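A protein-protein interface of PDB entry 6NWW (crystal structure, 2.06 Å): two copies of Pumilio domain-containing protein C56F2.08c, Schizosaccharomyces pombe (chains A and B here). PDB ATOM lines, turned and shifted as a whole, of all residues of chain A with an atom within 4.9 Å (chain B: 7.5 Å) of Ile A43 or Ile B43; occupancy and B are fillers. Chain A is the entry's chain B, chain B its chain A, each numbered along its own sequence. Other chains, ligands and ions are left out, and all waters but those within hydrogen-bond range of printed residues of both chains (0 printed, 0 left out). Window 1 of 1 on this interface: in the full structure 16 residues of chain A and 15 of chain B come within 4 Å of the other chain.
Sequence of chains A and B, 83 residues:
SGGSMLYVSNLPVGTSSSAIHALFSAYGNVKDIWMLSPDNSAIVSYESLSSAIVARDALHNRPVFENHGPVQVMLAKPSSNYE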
ATOM      1  N   MET A   5      -2.742 -29.994 -12.896  1.00  0.00           N
ATOM      2  CA  MET A   5      -3.381 -29.212 -13.949  1.00  0.00           C
ATOM      3  C   MET A   5      -2.608 -29.321 -15.257  1.00  0.00           C
ATOM      4  O   MET A   5      -1.392 -29.106 -15.288  1.00  0.00           O
ATOM      5  CB  MET A   5      -3.498 -27.742 -13.537  1.00  0.00           C
ATOM      6  CG  MET A   5      -4.342 -27.511 -12.290  1.00  0.00           C
ATOM      7  SD  MET A   5      -6.062 -27.992 -12.533  1.00  0.00           S
ATOM      8  CE  MET A   5      -6.700 -27.765 -10.877  1.00  0.00           C
ATOM      9  N   LEU A   6      -3.327 -29.626 -16.336  1.00  0.00           N
ATOM     10  CA  LEU A   6      -2.812 -29.530 -17.696  1.00  0.00           C
ATOM     11  C   LEU A   6      -3.542 -28.410 -18.426  1.00  0.00           C
ATOM     12  O   LEU A   6      -4.773 -28.325 -18.366  1.00  0.00           O
ATOM     13  CB  LEU A   6      -2.995 -30.842 -18.458  1.00  0.00           C
ATOM     14  CG  LEU A   6      -2.276 -32.085 -17.936  1.00  0.00           C
ATOM     15  CD1 LEU A   6      -2.582 -33.268 -18.830  1.00  0.00           C
ATOM     16  CD2 LEU A   6      -0.768 -31.844 -17.851  1.00  0.00           C
ATOM     17  N   TYR A   7      -2.789 -27.558 -19.111  1.00  0.00           N
ATOM     18  CA  TYR A   7      -3.358 -26.565 -20.014  1.00  0.00           C
ATOM     19  C   TYR A   7      -3.304 -27.132 -21.425  1.00  0.00           C
ATOM     20  O   TYR A   7      -2.215 -27.351 -21.970  1.00  0.00           O
ATOM     21  CB  TYR A   7      -2.608 -25.237 -19.928  1.00  0.00           C
ATOM     22  CG  TYR A   7      -3.049 -24.205 -20.945  1.00  0.00           C
ATOM     23  CD1 TYR A   7      -4.360 -23.729 -20.970  1.00  0.00           C
ATOM     24  CD2 TYR A   7      -2.150 -23.697 -21.878  1.00  0.00           C
ATOM     25  CE1 TYR A   7      -4.759 -22.780 -21.911  1.00  0.00           C
ATOM     26  CE2 TYR A   7      -2.539 -22.757 -22.811  1.00  0.00           C
ATOM     27  CZ  TYR A   7      -3.835 -22.299 -22.825  1.00  0.00           C
ATOM     28  OH  TYR A   7      -4.196 -21.365 -23.765  1.00  0.00           O
ATOM     29  N   ASP A  32     -11.716 -32.935 -13.161  1.00  0.00           N
ATOM     30  CA  ASP A  32     -12.456 -31.786 -13.646  1.00  0.00           C
ATOM     31  C   ASP A  32     -11.941 -31.416 -15.023  1.00  0.00           C
ATOM     32  O   ASP A  32     -10.779 -31.667 -15.361  1.00  0.00           O
ATOM     33  CB  ASP A  32     -12.315 -30.567 -12.724  1.00  0.00           C
ATOM     34  CG  ASP A  32     -13.069 -30.717 -11.414  1.00  0.00           C
ATOM     35  OD1 ASP A  32     -12.418 -30.944 -10.373  1.00  0.00           O
ATOM     36  OD2 ASP A  32     -14.310 -30.590 -11.425  1.00  0.00           O
ATOM     37  N   ILE A  33     -12.820 -30.814 -15.813  1.00  0.00           N
ATOM     38  CA  ILE A  33     -12.448 -30.167 -17.062  1.00  0.00           C
ATOM     39  C   ILE A  33     -13.105 -28.799 -17.074  1.00  0.00           C
ATOM     40  O   ILE A  33     -14.317 -28.687 -16.850  1.00  0.00           O
ATOM     41  CB  ILE A  33     -12.870 -30.994 -18.290  1.00  0.00           C
ATOM     42  CG1 ILE A  33     -12.087 -32.313 -18.323  1.00  0.00           C
ATOM     43  CG2 ILE A  33     -12.683 -30.184 -19.579  1.00  0.00           C
ATOM     44  CD1 ILE A  33     -12.633 -33.321 -19.294  1.00  0.00           C
ATOM     45  N   TRP A  34     -12.299 -27.760 -17.278  1.00  0.00           N
ATOM     46  CA  TRP A  34     -12.787 -26.406 -17.485  1.00  0.00           C
ATOM     47  C   TRP A  34     -12.511 -26.016 -18.930  1.00  0.00           C
ATOM     48  O   TRP A  34     -11.386 -26.178 -19.410  1.00  0.00           O
ATOM     49  CB  TRP A  34     -12.111 -25.411 -16.539  1.00  0.00           C
ATOM     50  CG  TRP A  34     -12.353 -25.643 -15.075  1.00  0.00           C
ATOM     51  CD1 TRP A  34     -13.311 -25.058 -14.294  1.00  0.00           C
ATOM     52  CD2 TRP A  34     -11.596 -26.492 -14.210  1.00  0.00           C
ATOM     53  NE1 TRP A  34     -13.203 -25.502 -12.998  1.00  0.00           N
ATOM     54  CE2 TRP A  34     -12.159 -26.386 -12.920  1.00  0.00           C
ATOM     55  CE3 TRP A  34     -10.496 -27.334 -14.398  1.00  0.00           C
ATOM     56  CZ2 TRP A  34     -11.658 -27.089 -11.827  1.00  0.00           C
ATOM     57  CZ3 TRP A  34     -10.000 -28.029 -13.312  1.00  0.00           C
ATOM     58  CH2 TRP A  34     -10.577 -27.897 -12.039  1.00  0.00           C
ATOM     59  N   LEU A  36     -12.180 -23.339 -22.143  1.00  0.00           N
ATOM     60  CA  LEU A  36     -11.830 -21.972 -22.530  1.00  0.00           C
ATOM     61  C   LEU A  36     -12.056 -21.855 -24.040  1.00  0.00           C
ATOM     62  O   LEU A  36     -11.116 -21.727 -24.826  1.00  0.00           O
ATOM     63  CB  LEU A  36     -10.390 -21.632 -22.144  1.00  0.00           C
ATOM     64  CG  LEU A  36      -9.995 -21.711 -20.664  1.00  0.00           C
ATOM     65  CD1 LEU A  36      -8.500 -21.971 -20.518  1.00  0.00           C
ATOM     66  CD2 LEU A  36     -10.392 -20.426 -19.937  1.00  0.00           C
ATOM     67  N   SER A  41      -9.210 -23.930 -26.035  1.00  0.00           N
ATOM     68  CA  SER A  41      -8.352 -24.530 -25.029  1.00  0.00           C
ATOM     69  C   SER A  41      -9.201 -25.021 -23.864  1.00  0.00           C
ATOM     70  O   SER A  41     -10.405 -24.758 -23.785  1.00  0.00           O
ATOM     71  CB  SER A  41      -7.279 -23.538 -24.562  1.00  0.00           C
ATOM     72  OG  SER A  41      -7.864 -22.479 -23.833  1.00  0.00           O
ATOM     73  N   ALA A  42      -8.555 -25.751 -22.958  1.00  0.00           N
ATOM     74  CA  ALA A  42      -9.234 -26.289 -21.790  1.00  0.00           C
ATOM     75  C   ALA A  42      -8.204 -26.561 -20.705  1.00  0.00           C
ATOM     76  O   ALA A  42      -6.997 -26.607 -20.961  1.00  0.00           O
ATOM     77  CB  ALA A  42     -10.015 -27.565 -22.124  1.00  0.00           C
ATOM     78  N   ILE A  43      -8.703 -26.730 -19.485  1.00  0.00           N
ATOM     79  CA  ILE A  43      -7.896 -27.093 -18.326  1.00  0.00           C
ATOM     80  C   ILE A  43      -8.379 -28.459 -17.861  1.00  0.00           C
ATOM     81  O   ILE A  43      -9.584 -28.662 -17.668  1.00  0.00           O
ATOM     82  CB  ILE A  43      -8.016 -26.052 -17.194  1.00  0.00           C
ATOM     83  CG1 ILE A  43      -7.484 -24.692 -17.646  1.00  0.00           C
ATOM     84  CG2 ILE A  43      -7.286 -26.528 -15.930  1.00  0.00           C
ATOM     85  CD1 ILE A  43      -7.806 -23.570 -16.673  1.00  0.00           C
ATOM     86  N   VAL A  44      -7.450 -29.393 -17.699  1.00  0.00           N
ATOM     87  CA  VAL A  44      -7.767 -30.758 -17.302  1.00  0.00           C
ATOM     88  C   VAL A  44      -7.066 -31.048 -15.987  1.00  0.00           C
ATOM     89  O   VAL A  44      -5.854 -30.840 -15.863  1.00  0.00           O
ATOM     90  CB  VAL A  44      -7.350 -31.774 -18.379  1.00  0.00           C
ATOM     91  CG1 VAL A  44      -7.706 -33.190 -17.934  1.00  0.00           C
ATOM     92  CG2 VAL A  44      -7.996 -31.425 -19.720  1.00  0.00           C
ATOM     93  N   SER A  45      -7.825 -31.534 -15.009  1.00  0.00           N
ATOM     94  CA  SER A  45      -7.299 -31.872 -13.697  1.00  0.00           C
ATOM     95  C   SER A  45      -7.348 -33.380 -13.492  1.00  0.00           C
ATOM     96  O   SER A  45      -8.400 -34.002 -13.683  1.00  0.00           O
ATOM     97  CB  SER A  45      -8.092 -31.169 -12.594  1.00  0.00           C
ATOM     98  OG  SER A  45      -7.572 -31.513 -11.328  1.00  0.00           O
ATOM     99  N   ALA A  76       1.169 -27.640 -15.743  1.00  0.00           N
ATOM    100  CA  ALA A  76       1.311 -26.434 -14.937  1.00  0.00           C
ATOM    101  C   ALA A  76       1.961 -26.768 -13.600  1.00  0.00           C
ATOM    102  O   ALA A  76       1.675 -27.804 -12.993  1.00  0.00           O
ATOM    103  CB  ALA A  76      -0.047 -25.771 -14.713  1.00  0.00           C
ATOM    104  N   SER B   4     -13.632 -21.000  -8.486  1.00  0.00           N
ATOM    105  CA  SER B   4     -13.603 -20.638  -9.898  1.00  0.00           C
ATOM    106  C   SER B   4     -12.180 -20.624 -10.427  1.00  0.00           C
ATOM    107  O   SER B   4     -11.236 -20.490  -9.659  1.00  0.00           O
ATOM    108  CB  SER B   4     -14.257 -19.278 -10.111  1.00  0.00           C
ATOM    109  OG  SER B   4     -15.658 -19.386  -9.944  1.00  0.00           O
ATOM    110  N   MET B   5     -12.035 -20.755 -11.745  1.00  0.00           N
ATOM    111  CA  MET B   5     -10.735 -20.852 -12.394  1.00  0.00           C
ATOM    112  C   MET B   5     -10.603 -19.768 -13.454  1.00  0.00           C
ATOM    113  O   MET B   5     -11.471 -19.630 -14.326  1.00  0.00           O
ATOM    114  CB  MET B   5     -10.537 -22.237 -13.019  1.00  0.00           C
ATOM    115  CG  MET B   5     -10.643 -23.372 -12.015  1.00  0.00           C
ATOM    116  SD  MET B   5      -9.103 -23.628 -11.123  1.00  0.00           S
ATOM    117  CE  MET B   5      -8.283 -24.758 -12.243  1.00  0.00           C
ATOM    118  N   LEU B   6      -9.523 -18.999 -13.364  1.00  0.00           N
ATOM    119  CA  LEU B   6      -9.182 -17.987 -14.350  1.00  0.00           C
ATOM    120  C   LEU B   6      -7.909 -18.403 -15.065  1.00  0.00           C
ATOM    121  O   LEU B   6      -6.946 -18.841 -14.427  1.00  0.00           O
ATOM    122  CB  LEU B   6      -8.970 -16.615 -13.705  1.00  0.00           C
ATOM    123  CG  LEU B   6     -10.115 -15.932 -12.956  1.00  0.00           C
ATOM    124  CD1 LEU B   6      -9.613 -14.617 -12.374  1.00  0.00           C
ATOM    125  CD2 LEU B   6     -11.313 -15.700 -13.870  1.00  0.00           C
ATOM    126  N   TYR B   7      -7.910 -18.264 -16.386  1.00  0.00           N
ATOM    127  CA  TYR B   7      -6.706 -18.410 -17.191  1.00  0.00           C
ATOM    128  C   TYR B   7      -6.157 -17.015 -17.469  1.00  0.00           C
ATOM    129  O   TYR B   7      -6.829 -16.191 -18.102  1.00  0.00           O
ATOM    130  CB  TYR B   7      -6.994 -19.156 -18.495  1.00  0.00           C
ATOM    131  CG  TYR B   7      -5.813 -19.212 -19.443  1.00  0.00           C
ATOM    132  CD1 TYR B   7      -4.667 -19.926 -19.114  1.00  0.00           C
ATOM    133  CD2 TYR B   7      -5.845 -18.550 -20.664  1.00  0.00           C
ATOM    134  CE1 TYR B   7      -3.580 -19.980 -19.979  1.00  0.00           C
ATOM    135  CE2 TYR B   7      -4.764 -18.597 -21.536  1.00  0.00           C
ATOM    136  CZ  TYR B   7      -3.635 -19.311 -21.186  1.00  0.00           C
ATOM    137  OH  TYR B   7      -2.559 -19.362 -22.042  1.00  0.00           O
ATOM    138  N   VAL B   8      -4.944 -16.754 -16.996  1.00  0.00           N
ATOM    139  CA  VAL B   8      -4.314 -15.443 -17.101  1.00  0.00           C
ATOM    140  C   VAL B   8      -3.136 -15.560 -18.051  1.00  0.00           C
ATOM    141  O   VAL B   8      -2.221 -16.359 -17.815  1.00  0.00           O
ATOM    142  CB  VAL B   8      -3.861 -14.927 -15.729  1.00  0.00           C
ATOM    143  CG1 VAL B   8      -3.390 -13.484 -15.835  1.00  0.00           C
ATOM    144  CG2 VAL B   8      -4.992 -15.075 -14.726  1.00  0.00           C
ATOM    145  N   SER B   9      -3.137 -14.743 -19.102  1.00  0.00           N
ATOM    146  CA  SER B   9      -2.112 -14.804 -20.134  1.00  0.00           C
ATOM    147  C   SER B   9      -1.524 -13.412 -20.347  1.00  0.00           C
ATOM    148  O   SER B   9      -1.955 -12.428 -19.735  1.00  0.00           O
ATOM    149  CB  SER B   9      -2.680 -15.377 -21.439  1.00  0.00           C
ATOM    150  OG  SER B   9      -3.721 -14.562 -21.953  1.00  0.00           O
ATOM    151  N   LEU B  11       1.330 -12.435 -19.371  1.00  0.00           N
ATOM    152  CA  LEU B  11       2.140 -12.007 -18.250  1.00  0.00           C
ATOM    153  C   LEU B  11       3.460 -11.446 -18.769  1.00  0.00           C
ATOM    154  O   LEU B  11       3.965 -11.889 -19.802  1.00  0.00           O
ATOM    155  CB  LEU B  11       2.418 -13.171 -17.303  1.00  0.00           C
ATOM    156  CG  LEU B  11       1.244 -13.912 -16.661  1.00  0.00           C
ATOM    157  CD1 LEU B  11       1.728 -15.200 -15.999  1.00  0.00           C
ATOM    158  CD2 LEU B  11       0.543 -13.013 -15.651  1.00  0.00           C
ATOM    159  N   ILE B  20       2.006 -12.668  -9.031  1.00  0.00           N
ATOM    160  CA  ILE B  20       0.642 -13.010  -9.432  1.00  0.00           C
ATOM    161  C   ILE B  20      -0.265 -13.090  -8.212  1.00  0.00           C
ATOM    162  O   ILE B  20      -1.378 -12.551  -8.205  1.00  0.00           O
ATOM    163  CB  ILE B  20       0.630 -14.332 -10.224  1.00  0.00           C
ATOM    164  CG1 ILE B  20       1.299 -14.144 -11.586  1.00  0.00           C
ATOM    165  CG2 ILE B  20      -0.797 -14.839 -10.386  1.00  0.00           C
ATOM    166  CD1 ILE B  20       1.479 -15.433 -12.349  1.00  0.00           C
ATOM    167  N   VAL B  30      -7.148 -15.914  -2.886  1.00  0.00           N
ATOM    168  CA  VAL B  30      -6.566 -16.802  -3.883  1.00  0.00           C
ATOM    169  C   VAL B  30      -6.347 -18.168  -3.248  1.00  0.00           C
ATOM    170  O   VAL B  30      -5.671 -18.289  -2.219  1.00  0.00           O
ATOM    171  CB  VAL B  30      -5.259 -16.217  -4.435  1.00  0.00           C
ATOM    172  CG1 VAL B  30      -4.576 -17.206  -5.374  1.00  0.00           C
ATOM    173  CG2 VAL B  30      -5.537 -14.901  -5.151  1.00  0.00           C
ATOM    174  N   ASP B  32      -5.266 -21.116  -5.174  1.00  0.00           N
ATOM    175  CA  ASP B  32      -4.114 -21.763  -5.790  1.00  0.00           C
ATOM    176  C   ASP B  32      -3.688 -20.958  -7.006  1.00  0.00           C
ATOM    177  O   ASP B  32      -4.485 -20.236  -7.606  1.00  0.00           O
ATOM    178  CB  ASP B  32      -4.421 -23.203  -6.213  1.00  0.00           C
ATOM    179  CG  ASP B  32      -4.470 -24.165  -5.046  1.00  0.00           C
ATOM    180  OD1 ASP B  32      -3.425 -24.355  -4.389  1.00  0.00           O
ATOM    181  OD2 ASP B  32      -5.551 -24.734  -4.791  1.00  0.00           O
ATOM    182  N   ILE B  33      -2.415 -21.105  -7.361  1.00  0.00           N
ATOM    183  CA  ILE B  33      -1.862 -20.589  -8.606  1.00  0.00           C
ATOM    184  C   ILE B  33      -1.029 -21.694  -9.235  1.00  0.00           C
ATOM    185  O   ILE B  33      -0.219 -22.325  -8.550  1.00  0.00           O
ATOM    186  CB  ILE B  33      -0.998 -19.333  -8.381  1.00  0.00           C
ATOM    187  CG1 ILE B  33      -1.862 -18.166  -7.905  1.00  0.00           C
ATOM    188  CG2 ILE B  33      -0.261 -18.948  -9.665  1.00  0.00           C
ATOM    189  CD1 ILE B  33      -1.050 -17.027  -7.370  1.00  0.00           C
ATOM    190  N   TRP B  34      -1.243 -21.942 -10.526  1.00  0.00           N
ATOM    191  CA  TRP B  34      -0.415 -22.860 -11.295  1.00  0.00           C
ATOM    192  C   TRP B  34       0.255 -22.074 -12.408  1.00  0.00           C
ATOM    193  O   TRP B  34      -0.425 -21.409 -13.195  1.00  0.00           O
ATOM    194  CB  TRP B  34      -1.233 -24.006 -11.889  1.00  0.00           C
ATOM    195  CG  TRP B  34      -1.916 -24.883 -10.889  1.00  0.00           C
ATOM    196  CD1 TRP B  34      -1.445 -26.052 -10.359  1.00  0.00           C
ATOM    197  CD2 TRP B  34      -3.213 -24.681 -10.322  1.00  0.00           C
ATOM    198  NE1 TRP B  34      -2.365 -26.579  -9.487  1.00  0.00           N
ATOM    199  CE2 TRP B  34      -3.460 -25.756  -9.448  1.00  0.00           C
ATOM    200  CE3 TRP B  34      -4.189 -23.691 -10.468  1.00  0.00           C
ATOM    201  CZ2 TRP B  34      -4.642 -25.869  -8.724  1.00  0.00           C
ATOM    202  CZ3 TRP B  34      -5.359 -23.804  -9.746  1.00  0.00           C
ATOM    203  CH2 TRP B  34      -5.577 -24.887  -8.888  1.00  0.00           C
ATOM    204  N   MET B  35       1.578 -22.156 -12.479  1.00  0.00           N
ATOM    205  CA  MET B  35       2.343 -21.373 -13.436  1.00  0.00           C
ATOM    206  C   MET B  35       2.515 -22.137 -14.744  1.00  0.00           C
ATOM    207  O   MET B  35       2.781 -23.341 -14.747  1.00  0.00           O
ATOM    208  CB  MET B  35       3.708 -21.008 -12.853  1.00  0.00           C
ATOM    209  CG  MET B  35       3.628 -20.217 -11.559  1.00  0.00           C
ATOM    210  SD  MET B  35       2.945 -18.571 -11.824  1.00  0.00           S
ATOM    211  CE  MET B  35       4.295 -17.797 -12.712  1.00  0.00           C
ATOM    212  N   LEU B  36       2.350 -21.419 -15.854  1.00  0.00           N
ATOM    213  CA  LEU B  36       2.628 -21.924 -17.197  1.00  0.00           C
ATOM    214  C   LEU B  36       3.610 -20.969 -17.880  1.00  0.00           C
ATOM    215  O   LEU B  36       3.317 -20.345 -18.901  1.00  0.00           O
ATOM    216  CB  LEU B  36       1.344 -22.060 -18.008  1.00  0.00           C
ATOM    217  CG  LEU B  36       0.261 -22.977 -17.449  1.00  0.00           C
ATOM    218  CD1 LEU B  36      -1.111 -22.461 -17.867  1.00  0.00           C
ATOM    219  CD2 LEU B  36       0.485 -24.390 -17.964  1.00  0.00           C
ATOM    220  N   SER B  41       1.867 -17.506 -18.905  1.00  0.00           N
ATOM    221  CA  SER B  41       0.484 -17.705 -18.495  1.00  0.00           C
ATOM    222  C   SER B  41       0.438 -18.314 -17.100  1.00  0.00           C
ATOM    223  O   SER B  41       1.437 -18.809 -16.579  1.00  0.00           O
ATOM    224  CB  SER B  41      -0.263 -18.632 -19.460  1.00  0.00           C
ATOM    225  OG  SER B  41      -0.685 -17.943 -20.619  1.00  0.00           O
ATOM    226  N   ALA B  42      -0.754 -18.304 -16.517  1.00  0.00           N
ATOM    227  CA  ALA B  42      -0.977 -18.900 -15.209  1.00  0.00           C
ATOM    228  C   ALA B  42      -2.453 -19.243 -15.084  1.00  0.00           C
ATOM    229  O   ALA B  42      -3.299 -18.714 -15.810  1.00  0.00           O
ATOM    230  CB  ALA B  42      -0.538 -17.965 -14.075  1.00  0.00           C
ATOM    231  N   ILE B  43      -2.741 -20.164 -14.169  1.00  0.00           N
ATOM    232  CA  ILE B  43      -4.099 -20.498 -13.763  1.00  0.00           C
ATOM    233  C   ILE B  43      -4.249 -20.055 -12.316  1.00  0.00           C
ATOM    234  O   ILE B  43      -3.419 -20.410 -11.467  1.00  0.00           O
ATOM    235  CB  ILE B  43      -4.384 -22.003 -13.912  1.00  0.00           C
ATOM    236  CG1 ILE B  43      -4.176 -22.461 -15.357  1.00  0.00           C
ATOM    237  CG2 ILE B  43      -5.789 -22.346 -13.420  1.00  0.00           C
ATOM    238  CD1 ILE B  43      -4.132 -23.971 -15.503  1.00  0.00           C
ATOM    239  N   VAL B  44      -5.280 -19.263 -12.034  1.00  0.00           N
ATOM    240  CA  VAL B  44      -5.537 -18.778 -10.683  1.00  0.00           C
ATOM    241  C   VAL B  44      -6.935 -19.223 -10.270  1.00  0.00           C
ATOM    242  O   VAL B  44      -7.887 -19.134 -11.058  1.00  0.00           O
ATOM    243  CB  VAL B  44      -5.366 -17.249 -10.573  1.00  0.00           C
ATOM    244  CG1 VAL B  44      -5.764 -16.756  -9.170  1.00  0.00           C
ATOM    245  CG2 VAL B  44      -3.948 -16.808 -10.917  1.00  0.00           C
ATOM    246  N   SER B  45      -7.051 -19.735  -9.047  1.00  0.00           N
ATOM    247  CA  SER B  45      -8.326 -20.190  -8.507  1.00  0.00           C
ATOM    248  C   SER B  45      -8.694 -19.371  -7.277  1.00  0.00           C
ATOM    249  O   SER B  45      -7.865 -19.173  -6.381  1.00  0.00           O
ATOM    250  CB  SER B  45      -8.279 -21.677  -8.153  1.00  0.00           C
ATOM    251  OG  SER B  45      -7.409 -21.907  -7.061  1.00  0.00           O
ATOM    252  N   MET B  74      -9.376 -14.761 -18.696  1.00  0.00           N
ATOM    253  CA  MET B  74     -10.544 -15.476 -19.189  1.00  0.00           C
ATOM    254  C   MET B  74     -11.063 -16.391 -18.092  1.00  0.00           C
ATOM    255  O   MET B  74     -10.288 -17.128 -17.474  1.00  0.00           O
ATOM    256  CB  MET B  74     -10.212 -16.285 -20.454  1.00  0.00           C
ATOM    257  CG  MET B  74     -11.374 -17.114 -20.986  1.00  0.00           C
ATOM    258  SD  MET B  74     -11.075 -17.837 -22.624  1.00  0.00           S
ATOM    259  CE  MET B  74     -10.897 -16.352 -23.615  1.00  0.00           C
ATOM    260  N   LEU B  75     -12.368 -16.332 -17.845  1.00  0.00           N
ATOM    261  CA  LEU B  75     -13.004 -17.200 -16.864  1.00  0.00           C
ATOM    262  C   LEU B  75     -13.257 -18.574 -17.480  1.00  0.00           C
ATOM    263  O   LEU B  75     -13.955 -18.685 -18.492  1.00  0.00           O
ATOM    264  CB  LEU B  75     -14.311 -16.578 -16.386  1.00  0.00           C
ATOM    265  CG  LEU B  75     -15.205 -17.433 -15.492  1.00  0.00           C
ATOM    266  CD1 LEU B  75     -14.521 -17.696 -14.150  1.00  0.00           C
ATOM    267  CD2 LEU B  75     -16.561 -16.749 -15.291  1.00  0.00           C
ATOM    268  N   ALA B  76     -12.703 -19.615 -16.863  1.00  0.00           N
ATOM    269  CA  ALA B  76     -12.863 -20.983 -17.351  1.00  0.00           C
ATOM    270  C   ALA B  76     -14.170 -21.580 -16.838  1.00  0.00           C
ATOM    271  O   ALA B  76     -14.376 -21.678 -15.624  1.00  0.00           O
ATOM    272  CB  ALA B  76     -11.673 -21.836 -16.910  1.00  0.00           C
ATOM    273  N   LYS B  77     -15.043 -22.005 -17.750  1.00  0.00           N
ATOM    274  CA  LYS B  77     -16.322 -22.567 -17.337  1.00  0.00           C
ATOM    275  C   LYS B  77     -16.145 -24.021 -16.915  1.00  0.00           C
ATOM    276  O   LYS B  77     -15.622 -24.826 -17.700  1.00  0.00           O
ATOM    277  CB  LYS B  77     -17.365 -22.455 -18.447  1.00  0.00           C
ATOM    278  CG  LYS B  77     -17.052 -23.200 -19.736  1.00  0.00           C
ATOM    279  CD  LYS B  77     -18.173 -23.007 -20.761  1.00  0.00           C
ATOM    280  CE  LYS B  77     -17.850 -23.750 -22.032  1.00  0.00           C
ATOM    281  NZ  LYS B  77     -16.651 -23.155 -22.661  1.00  0.00           N
ATOM    282  N   SER B  79     -17.268 -27.922 -16.138  1.00  0.00           N
ATOM    283  CA  SER B  79     -18.194 -28.854 -16.767  1.00  0.00           C
ATOM    284  C   SER B  79     -18.332 -30.110 -15.912  1.00  0.00           C
ATOM    285  O   SER B  79     -17.633 -31.100 -16.121  1.00  0.00           O
ATOM    286  CB  SER B  79     -17.729 -29.210 -18.182  1.00  0.00           C
ATOM    287  OG  SER B  79     -16.449 -29.818 -18.169  1.00  0.00           O
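Met A5 touches its own counterpart, Met B5. Tyr A7 touches Leu B36, and with the chains exchanged Leu A36 touches Tyr B7. Trp A34 touches Ala B76, and with the chains exchanged Ala A76 touches Trp B34. Ile A43 touches its own counterpart, Ile B43.
The backbone NH (N) of Ala B76 lies within hydrogen-bond range of the backbone carbonyl oxygen (O) of Met B5, 2.8 Å away. The side-chain hydroxyl of Ser B41 sits at hydrogen-bond distance from the side-chain hydroxyl of Tyr B7 (2.7 Å). The backbone carbonyl oxygen (O) of Trp B34 sits at hydrogen-bond distance from the backbone NH (N) of Ile B43 (2.8 Å). O of Met A5 is in hydrogen-bond range of N of Ala A76 (3.0 Å). N of Ile A43 is in hydrogen-bond range of O of Trp A34, at 2.7 Å. N of Leu A36 is in hydrogen-bond range of O of Ser A41, at 2.8 Å.
Of the 24 printed residues of chain B, 10 touch a printed residue of chain A. Hydrophobic or aromatic side chains of chain B within 4 Å of the printed part of chain A: Met B5, Tyr B7, Trp B34, Leu B36, Ile B43, Met B74 and Ala B76. Along chain B the printed residues that touch a printed residue of chain A span positions 5 to 79. Of the 13 printed residues of chain A, 7 touch a printed residue of chain B.
Ile A43 touches one residue of chain B. Printed residues of chain A within 4 Å of Met B74: Leu A36 (3.6 Å). Of the printed residues of chain A, Trp B34 touches Met A5 (3.5 Å) and Ala A76 (3.5 Å). The nearest residue of chain A that does not touch Ile B43 is Met A5 (4.3 Å). The nearest printed residue of chain B that does not touch Tyr A7 is Ile B43 (4.8 Å).
Met A5 touches Trp B34 (CG to CE2, 3.5 Å). Leu B36 touches Tyr A7 (CD2 to CB, 3.8 Å). CB of Trp A34 touches CB of Ala B76 (3.6 Å). O of Lys B77 touches CA of Trp A34, 3.3 Å away. Leu A36 touches Tyr B7 (CD1 to CB, 3.8 Å). CB of Ala B76 touches CD2 of Leu A36 (3.6 Å). CD1 of Ile B43 touches CD1 of Ile A43 (3.9 Å). Ala A76 touches Trp B34. Met B35 touches Ala A76 (O to CA, 3.4 Å). Leu B36 touches Ala A76.
The side-chain hydroxyl (OH) of Tyr B7 lies within hydrogen-bond range of the side-chain hydroxyl (OH) of Tyr A7. O of Ile A33 lies within hydrogen-bond range of OG of Ser B79, 2.8 Å away.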
